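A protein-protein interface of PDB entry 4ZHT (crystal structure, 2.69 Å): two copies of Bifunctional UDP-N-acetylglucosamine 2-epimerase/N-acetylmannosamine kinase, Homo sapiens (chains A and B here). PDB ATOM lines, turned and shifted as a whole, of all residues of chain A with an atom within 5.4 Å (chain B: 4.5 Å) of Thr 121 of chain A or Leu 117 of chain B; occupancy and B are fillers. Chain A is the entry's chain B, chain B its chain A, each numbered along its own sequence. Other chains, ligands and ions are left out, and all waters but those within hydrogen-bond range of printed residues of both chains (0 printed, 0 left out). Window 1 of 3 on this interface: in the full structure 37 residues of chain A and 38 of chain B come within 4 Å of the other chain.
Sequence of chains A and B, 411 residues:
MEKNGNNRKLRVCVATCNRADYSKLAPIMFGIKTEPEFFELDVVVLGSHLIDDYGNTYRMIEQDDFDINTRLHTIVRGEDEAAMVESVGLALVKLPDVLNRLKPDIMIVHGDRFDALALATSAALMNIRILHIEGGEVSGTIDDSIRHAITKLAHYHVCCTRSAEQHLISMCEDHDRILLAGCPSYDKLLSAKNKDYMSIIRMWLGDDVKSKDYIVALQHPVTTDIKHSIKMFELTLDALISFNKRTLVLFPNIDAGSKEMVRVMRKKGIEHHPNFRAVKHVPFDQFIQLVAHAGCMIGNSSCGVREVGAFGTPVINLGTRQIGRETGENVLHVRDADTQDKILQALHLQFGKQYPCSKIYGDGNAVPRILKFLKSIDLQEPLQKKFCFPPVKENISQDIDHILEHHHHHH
O of Leu 117 of chain B sits at hydrogen-bond distance from OG1 of Thr 121 of chain B (2.6 Å). O of Leu 117 of chain A is in hydrogen-bond range of OG1 of Thr 121 of chain A (2.6 Å).
Leu 117 of chain A touches Thr 121 of chain B (CD2 to CG2, 3.8 Å). CG2 of Thr 121 of chain A touches CD2 of Leu 117 of chain B (3.7 Å). Leu 125 of chain A touches Ile 146 of chain B (CD2 to CD1, 3.8 Å).
Of the printed residues of chain B, Thr 121 of chain A touches Leu 117. Of chain A, only Thr 121 comes within 4 Å of Leu 117 of chain B. Printed residues of chain B within 4 Å of Leu 117 of chain A: Thr 121 (3.8 Å). Of the printed residues of chain A, Ile 146 of chain B touches Leu 125. Printed residues of chain A within 4 Å of Thr 121 of chain B: Leu 117. Of the printed residues of chain B, Leu 125 of chain A touches Ile 146 (3.8 Å). Leu 153 of chain B touches none of the printed residues of chain A. The nearest printed residue of chain B that does not touch Thr 121 of chain A is Thr 121 of chain B (5.9 Å). The nearest residue of chain A that does not touch Leu 117 of chain B is Leu 153 of chain A (5.0 Å). The nearest printed residue of chain A that does not touch Ile 146 of chain B is Leu 153 of chain A (4.02 Å).
Printed residues of chain A that touch a printed residue of chain B: Leu 117, Thr 121 and Leu 125. Hydrophobic or aromatic side chains of chain A that line the printed part of chain B: Leu 117 and Leu 125. Along chain A the printed residues that touch a printed residue of chain B span positions 117 to 125. Of the 12 printed residues of chain B, 3 touch a printed residue of chain A. Hydrophobic or aromatic side chains of chain B within 4 Å of the printed part of chain A: Leu 117 and Ile 146. Among the printed residues, 3 pairs touch across the chains. Among the printed residues, no Asp or Glu carboxylate lies within 4 Å of a Lys or Arg side-chain nitrogen of the other chain.
Leu 117 of chain A touches Thr 121 of chain B, and with the chains exchanged Thr 121 of chain A touches Leu 117 of chain B. Positions printed for both chains: 116, 117, 118, 119, 120, 121 and 153.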
ATOM      1  N   LEU A  92       4.079  11.282 -22.362  1.00  0.00           N
ATOM      2  CA  LEU A  92       5.512  11.536 -22.220  1.00  0.00           C
ATOM      3  C   LEU A  92       6.308  10.340 -21.735  1.00  0.00           C
ATOM      4  O   LEU A  92       7.457  10.210 -22.139  1.00  0.00           O
ATOM      5  CB  LEU A  92       5.783  12.740 -21.339  1.00  0.00           C
ATOM      6  CG  LEU A  92       5.480  14.110 -21.961  1.00  0.00           C
ATOM      7  CD1 LEU A  92       5.822  15.156 -20.914  1.00  0.00           C
ATOM      8  CD2 LEU A  92       6.277  14.382 -23.230  1.00  0.00           C
ATOM      9  N   ALA A 116      -0.916  17.901 -27.815  1.00  0.00           N
ATOM     10  CA  ALA A 116       0.104  18.459 -28.725  1.00  0.00           C
ATOM     11  C   ALA A 116       1.325  18.983 -27.975  1.00  0.00           C
ATOM     12  O   ALA A 116       2.448  18.962 -28.498  1.00  0.00           O
ATOM     13  CB  ALA A 116      -0.478  19.569 -29.563  1.00  0.00           C
ATOM     14  N   LEU A 117       1.113  19.440 -26.743  1.00  0.00           N
ATOM     15  CA  LEU A 117       2.215  19.903 -25.907  1.00  0.00           C
ATOM     16  C   LEU A 117       3.101  18.726 -25.497  1.00  0.00           C
ATOM     17  O   LEU A 117       4.309  18.874 -25.377  1.00  0.00           O
ATOM     18  CB  LEU A 117       1.672  20.665 -24.706  1.00  0.00           C
ATOM     19  CG  LEU A 117       2.698  21.158 -23.707  1.00  0.00           C
ATOM     20  CD1 LEU A 117       3.669  22.133 -24.323  1.00  0.00           C
ATOM     21  CD2 LEU A 117       1.979  21.775 -22.536  1.00  0.00           C
ATOM     22  N   ALA A 118       2.498  17.560 -25.285  1.00  0.00           N
ATOM     23  CA  ALA A 118       3.265  16.346 -24.991  1.00  0.00           C
ATOM     24  C   ALA A 118       4.145  15.964 -26.149  1.00  0.00           C
ATOM     25  O   ALA A 118       5.330  15.631 -25.974  1.00  0.00           O
ATOM     26  CB  ALA A 118       2.338  15.176 -24.654  1.00  0.00           C
ATOM     27  N   LEU A 119       3.548  15.983 -27.336  1.00  0.00           N
ATOM     28  CA  LEU A 119       4.276  15.651 -28.557  1.00  0.00           C
ATOM     29  C   LEU A 119       5.422  16.621 -28.816  1.00  0.00           C
ATOM     30  O   LEU A 119       6.540  16.199 -29.065  1.00  0.00           O
ATOM     31  CB  LEU A 119       3.326  15.616 -29.744  1.00  0.00           C
ATOM     32  CG  LEU A 119       2.410  14.401 -29.696  1.00  0.00           C
ATOM     33  CD1 LEU A 119       1.154  14.631 -30.520  1.00  0.00           C
ATOM     34  CD2 LEU A 119       3.139  13.154 -30.187  1.00  0.00           C
ATOM     35  N   ALA A 120       5.141  17.912 -28.737  1.00  0.00           N
ATOM     36  CA  ALA A 120       6.173  18.928 -28.949  1.00  0.00           C
ATOM     37  C   ALA A 120       7.296  18.794 -27.939  1.00  0.00           C
ATOM     38  O   ALA A 120       8.469  18.855 -28.293  1.00  0.00           O
ATOM     39  CB  ALA A 120       5.579  20.332 -28.881  1.00  0.00           C
ATOM     40  N   THR A 121       6.925  18.570 -26.687  1.00  0.00           N
ATOM     41  CA  THR A 121       7.905  18.448 -25.617  1.00  0.00           C
ATOM     42  C   THR A 121       8.856  17.277 -25.865  1.00  0.00           C
ATOM     43  O   THR A 121      10.085  17.437 -25.795  1.00  0.00           O
ATOM     44  CB  THR A 121       7.220  18.272 -24.249  1.00  0.00           C
ATOM     45  OG1 THR A 121       6.425  19.422 -23.984  1.00  0.00           O
ATOM     46  CG2 THR A 121       8.246  18.127 -23.129  1.00  0.00           C
ATOM     47  N   SER A 122       8.279  16.131 -26.195  1.00  0.00           N
ATOM     48  CA  SER A 122       9.056  14.932 -26.376  1.00  0.00           C
ATOM     49  C   SER A 122       9.987  15.054 -27.587  1.00  0.00           C
ATOM     50  O   SER A 122      11.171  14.764 -27.481  1.00  0.00           O
ATOM     51  CB  SER A 122       8.125  13.709 -26.475  1.00  0.00           C
ATOM     52  OG  SER A 122       7.459  13.673 -27.710  1.00  0.00           O
ATOM     53  N   ALA A 123       9.479  15.570 -28.700  1.00  0.00           N
ATOM     54  CA  ALA A 123      10.322  15.830 -29.877  1.00  0.00           C
ATOM     55  C   ALA A 123      11.473  16.801 -29.618  1.00  0.00           C
ATOM     56  O   ALA A 123      12.621  16.511 -29.973  1.00  0.00           O
ATOM     57  CB  ALA A 123       9.487  16.345 -31.016  1.00  0.00           C
ATOM     58  N   ALA A 124      11.153  17.931 -29.002  1.00  0.00           N
ATOM     59  CA  ALA A 124      12.135  18.985 -28.751  1.00  0.00           C
ATOM     60  C   ALA A 124      13.245  18.488 -27.853  1.00  0.00           C
ATOM     61  O   ALA A 124      14.402  18.744 -28.109  1.00  0.00           O
ATOM     62  CB  ALA A 124      11.475  20.193 -28.120  1.00  0.00           C
ATOM     63  N   LEU A 125      12.894  17.803 -26.777  1.00  0.00           N
ATOM     64  CA  LEU A 125      13.913  17.353 -25.835  1.00  0.00           C
ATOM     65  C   LEU A 125      14.757  16.191 -26.386  1.00  0.00           C
ATOM     66  O   LEU A 125      15.836  15.929 -25.877  1.00  0.00           O
ATOM     67  CB  LEU A 125      13.282  16.986 -24.506  1.00  0.00           C
ATOM     68  CG  LEU A 125      12.816  18.177 -23.686  1.00  0.00           C
ATOM     69  CD1 LEU A 125      11.967  17.682 -22.529  1.00  0.00           C
ATOM     70  CD2 LEU A 125      13.991  18.967 -23.119  1.00  0.00           C
ATOM     71  N   MET A 126      14.266  15.511 -27.427  1.00  0.00           N
ATOM     72  CA  MET A 126      15.020  14.435 -28.085  1.00  0.00           C
ATOM     73  C   MET A 126      15.670  14.860 -29.360  1.00  0.00           C
ATOM     74  O   MET A 126      16.142  14.023 -30.119  1.00  0.00           O
ATOM     75  CB  MET A 126      14.067  13.271 -28.326  1.00  0.00           C
ATOM     76  CG  MET A 126      13.732  12.691 -26.956  1.00  0.00           C
ATOM     77  SD  MET A 126      12.742  11.072 -27.263  1.00  0.00           S
ATOM     78  CE  MET A 126      10.978  11.862 -27.269  1.00  0.00           C
ATOM     79  N   LEU A 153       8.730  25.700 -28.654  1.00  0.00           N
ATOM     80  CA  LEU A 153       9.450  24.425 -28.767  1.00  0.00           C
ATOM     81  C   LEU A 153       9.739  24.085 -30.224  1.00  0.00           C
ATOM     82  O   LEU A 153      10.816  23.578 -30.539  1.00  0.00           O
ATOM     83  CB  LEU A 153       8.633  23.309 -28.137  1.00  0.00           C
ATOM     84  CG  LEU A 153       8.310  23.519 -26.668  1.00  0.00           C
ATOM     85  CD1 LEU A 153       7.317  22.473 -26.196  1.00  0.00           C
ATOM     86  CD2 LEU A 153       9.570  23.470 -25.823  1.00  0.00           C
ATOM     87  N   ARG B 113      15.115  24.034 -16.923  1.00  0.00           N
ATOM     88  CA  ARG B 113      15.297  22.591 -16.999  1.00  0.00           C
ATOM     89  C   ARG B 113      13.979  21.841 -17.280  1.00  0.00           C
ATOM     90  O   ARG B 113      12.885  22.341 -16.992  1.00  0.00           O
ATOM     91  CB  ARG B 113      15.930  22.097 -15.715  1.00  0.00           C
ATOM     92  CG  ARG B 113      17.380  22.487 -15.639  1.00  0.00           C
ATOM     93  CD  ARG B 113      17.987  22.220 -14.288  1.00  0.00           C
ATOM     94  NE  ARG B 113      19.405  22.505 -14.366  1.00  0.00           N
ATOM     95  CZ  ARG B 113      20.403  21.628 -14.256  1.00  0.00           C
ATOM     96  NH1 ARG B 113      20.184  20.337 -13.989  1.00  0.00           N
ATOM     97  NH2 ARG B 113      21.668  22.079 -14.378  1.00  0.00           N
ATOM     98  N   PHE B 114      14.114  20.619 -17.816  1.00  0.00           N
ATOM     99  CA  PHE B 114      12.971  19.773 -18.175  1.00  0.00           C
ATOM    100  C   PHE B 114      11.957  19.664 -17.051  1.00  0.00           C
ATOM    101  O   PHE B 114      10.760  19.778 -17.286  1.00  0.00           O
ATOM    102  CB  PHE B 114      13.436  18.393 -18.661  1.00  0.00           C
ATOM    103  CG  PHE B 114      14.003  17.492 -17.588  1.00  0.00           C
ATOM    104  CD1 PHE B 114      13.162  16.682 -16.801  1.00  0.00           C
ATOM    105  CD2 PHE B 114      15.381  17.394 -17.389  1.00  0.00           C
ATOM    106  CE1 PHE B 114      13.673  15.837 -15.820  1.00  0.00           C
ATOM    107  CE2 PHE B 114      15.901  16.525 -16.422  1.00  0.00           C
ATOM    108  CZ  PHE B 114      15.049  15.744 -15.638  1.00  0.00           C
ATOM    109  N   ASP B 115      12.462  19.516 -15.824  1.00  0.00           N
ATOM    110  CA  ASP B 115      11.653  19.452 -14.601  1.00  0.00           C
ATOM    111  C   ASP B 115      10.743  20.668 -14.409  1.00  0.00           C
ATOM    112  O   ASP B 115       9.626  20.518 -13.976  1.00  0.00           O
ATOM    113  CB  ASP B 115      12.580  19.340 -13.371  1.00  0.00           C
ATOM    114  CG  ASP B 115      12.931  17.892 -12.996  1.00  0.00           C
ATOM    115  OD1 ASP B 115      12.024  17.071 -12.673  1.00  0.00           O
ATOM    116  OD2 ASP B 115      14.145  17.591 -13.003  1.00  0.00           O
ATOM    117  N   ALA B 116      11.244  21.876 -14.686  1.00  0.00           N
ATOM    118  CA  ALA B 116      10.443  23.116 -14.541  1.00  0.00           C
ATOM    119  C   ALA B 116       9.307  23.210 -15.540  1.00  0.00           C
ATOM    120  O   ALA B 116       8.264  23.787 -15.256  1.00  0.00           O
ATOM    121  CB  ALA B 116      11.324  24.334 -14.690  1.00  0.00           C
ATOM    122  N   LEU B 117       9.497  22.599 -16.700  1.00  0.00           N
ATOM    123  CA  LEU B 117       8.452  22.541 -17.704  1.00  0.00           C
ATOM    124  C   LEU B 117       7.300  21.632 -17.267  1.00  0.00           C
ATOM    125  O   LEU B 117       6.145  21.914 -17.552  1.00  0.00           O
ATOM    126  CB  LEU B 117       9.034  22.097 -19.053  1.00  0.00           C
ATOM    127  CG  LEU B 117       8.034  21.945 -20.194  1.00  0.00           C
ATOM    128  CD1 LEU B 117       7.349  23.255 -20.525  1.00  0.00           C
ATOM    129  CD2 LEU B 117       8.749  21.382 -21.394  1.00  0.00           C
ATOM    130  N   ALA B 118       7.620  20.565 -16.547  1.00  0.00           N
ATOM    131  CA  ALA B 118       6.594  19.703 -15.950  1.00  0.00           C
ATOM    132  C   ALA B 118       5.766  20.449 -14.933  1.00  0.00           C
ATOM    133  O   ALA B 118       4.523  20.358 -14.924  1.00  0.00           O
ATOM    134  CB  ALA B 118       7.227  18.497 -15.278  1.00  0.00           C
ATOM    135  N   LEU B 119       6.463  21.175 -14.064  1.00  0.00           N
ATOM    136  CA  LEU B 119       5.800  21.960 -13.028  1.00  0.00           C
ATOM    137  C   LEU B 119       4.917  23.056 -13.627  1.00  0.00           C
ATOM    138  O   LEU B 119       3.747  23.174 -13.244  1.00  0.00           O
ATOM    139  CB  LEU B 119       6.824  22.571 -12.080  1.00  0.00           C
ATOM    140  CG  LEU B 119       7.468  21.521 -11.186  1.00  0.00           C
ATOM    141  CD1 LEU B 119       8.811  21.975 -10.672  1.00  0.00           C
ATOM    142  CD2 LEU B 119       6.538  21.173 -10.027  1.00  0.00           C
ATOM    143  N   ALA B 120       5.448  23.815 -14.584  1.00  0.00           N
ATOM    144  CA  ALA B 120       4.673  24.853 -15.221  1.00  0.00           C
ATOM    145  C   ALA B 120       3.455  24.281 -15.918  1.00  0.00           C
ATOM    146  O   ALA B 120       2.359  24.834 -15.834  1.00  0.00           O
ATOM    147  CB  ALA B 120       5.536  25.634 -16.205  1.00  0.00           C
ATOM    148  N   THR B 121       3.636  23.156 -16.589  1.00  0.00           N
ATOM    149  CA  THR B 121       2.563  22.544 -17.363  1.00  0.00           C
ATOM    150  C   THR B 121       1.433  22.157 -16.457  1.00  0.00           C
ATOM    151  O   THR B 121       0.258  22.452 -16.739  1.00  0.00           O
ATOM    152  CB  THR B 121       3.078  21.320 -18.159  1.00  0.00           C
ATOM    153  OG1 THR B 121       4.072  21.754 -19.097  1.00  0.00           O
ATOM    154  CG2 THR B 121       1.960  20.634 -18.940  1.00  0.00           C
ATOM    155  N   ILE B 146      13.023  25.759 -23.759  1.00  0.00           N
ATOM    156  CA  ILE B 146      12.297  25.350 -22.578  1.00  0.00           C
ATOM    157  C   ILE B 146      11.980  26.581 -21.772  1.00  0.00           C
ATOM    158  O   ILE B 146      10.848  26.757 -21.328  1.00  0.00           O
ATOM    159  CB  ILE B 146      13.110  24.370 -21.698  1.00  0.00           C
ATOM    160  CG1 ILE B 146      13.660  23.198 -22.492  1.00  0.00           C
ATOM    161  CG2 ILE B 146      12.251  23.821 -20.575  1.00  0.00           C
ATOM    162  CD1 ILE B 146      12.647  22.529 -23.412  1.00  0.00           C
ATOM    163  N   ILE B 150       8.144  27.853 -20.855  1.00  0.00           N
ATOM    164  CA  ILE B 150       7.696  28.100 -19.492  1.00  0.00           C
ATOM    165  C   ILE B 150       7.149  29.533 -19.299  1.00  0.00           C
ATOM    166  O   ILE B 150       6.098  29.725 -18.689  1.00  0.00           O
ATOM    167  CB  ILE B 150       8.810  27.816 -18.484  1.00  0.00           C
ATOM    168  CG1 ILE B 150       9.113  26.314 -18.472  1.00  0.00           C
ATOM    169  CG2 ILE B 150       8.409  28.263 -17.076  1.00  0.00           C
ATOM    170  CD1 ILE B 150      10.412  25.961 -17.792  1.00  0.00           C
ATOM    171  N   LEU B 153       3.586  29.808 -20.407  1.00  0.00           N
ATOM    172  CA  LEU B 153       2.627  29.165 -19.506  1.00  0.00           C
ATOM    173  C   LEU B 153       2.403  30.023 -18.286  1.00  0.00           C
ATOM    174  O   LEU B 153       1.273  30.117 -17.792  1.00  0.00           O
ATOM    175  CB  LEU B 153       3.125  27.787 -19.097  1.00  0.00           C
ATOM    176  CG  LEU B 153       3.349  26.813 -20.250  1.00  0.00           C
ATOM    177  CD1 LEU B 153       4.047  25.561 -19.747  1.00  0.00           C
ATOM    178  CD2 LEU B 153       2.043  26.448 -20.931  1.00  0.00           C
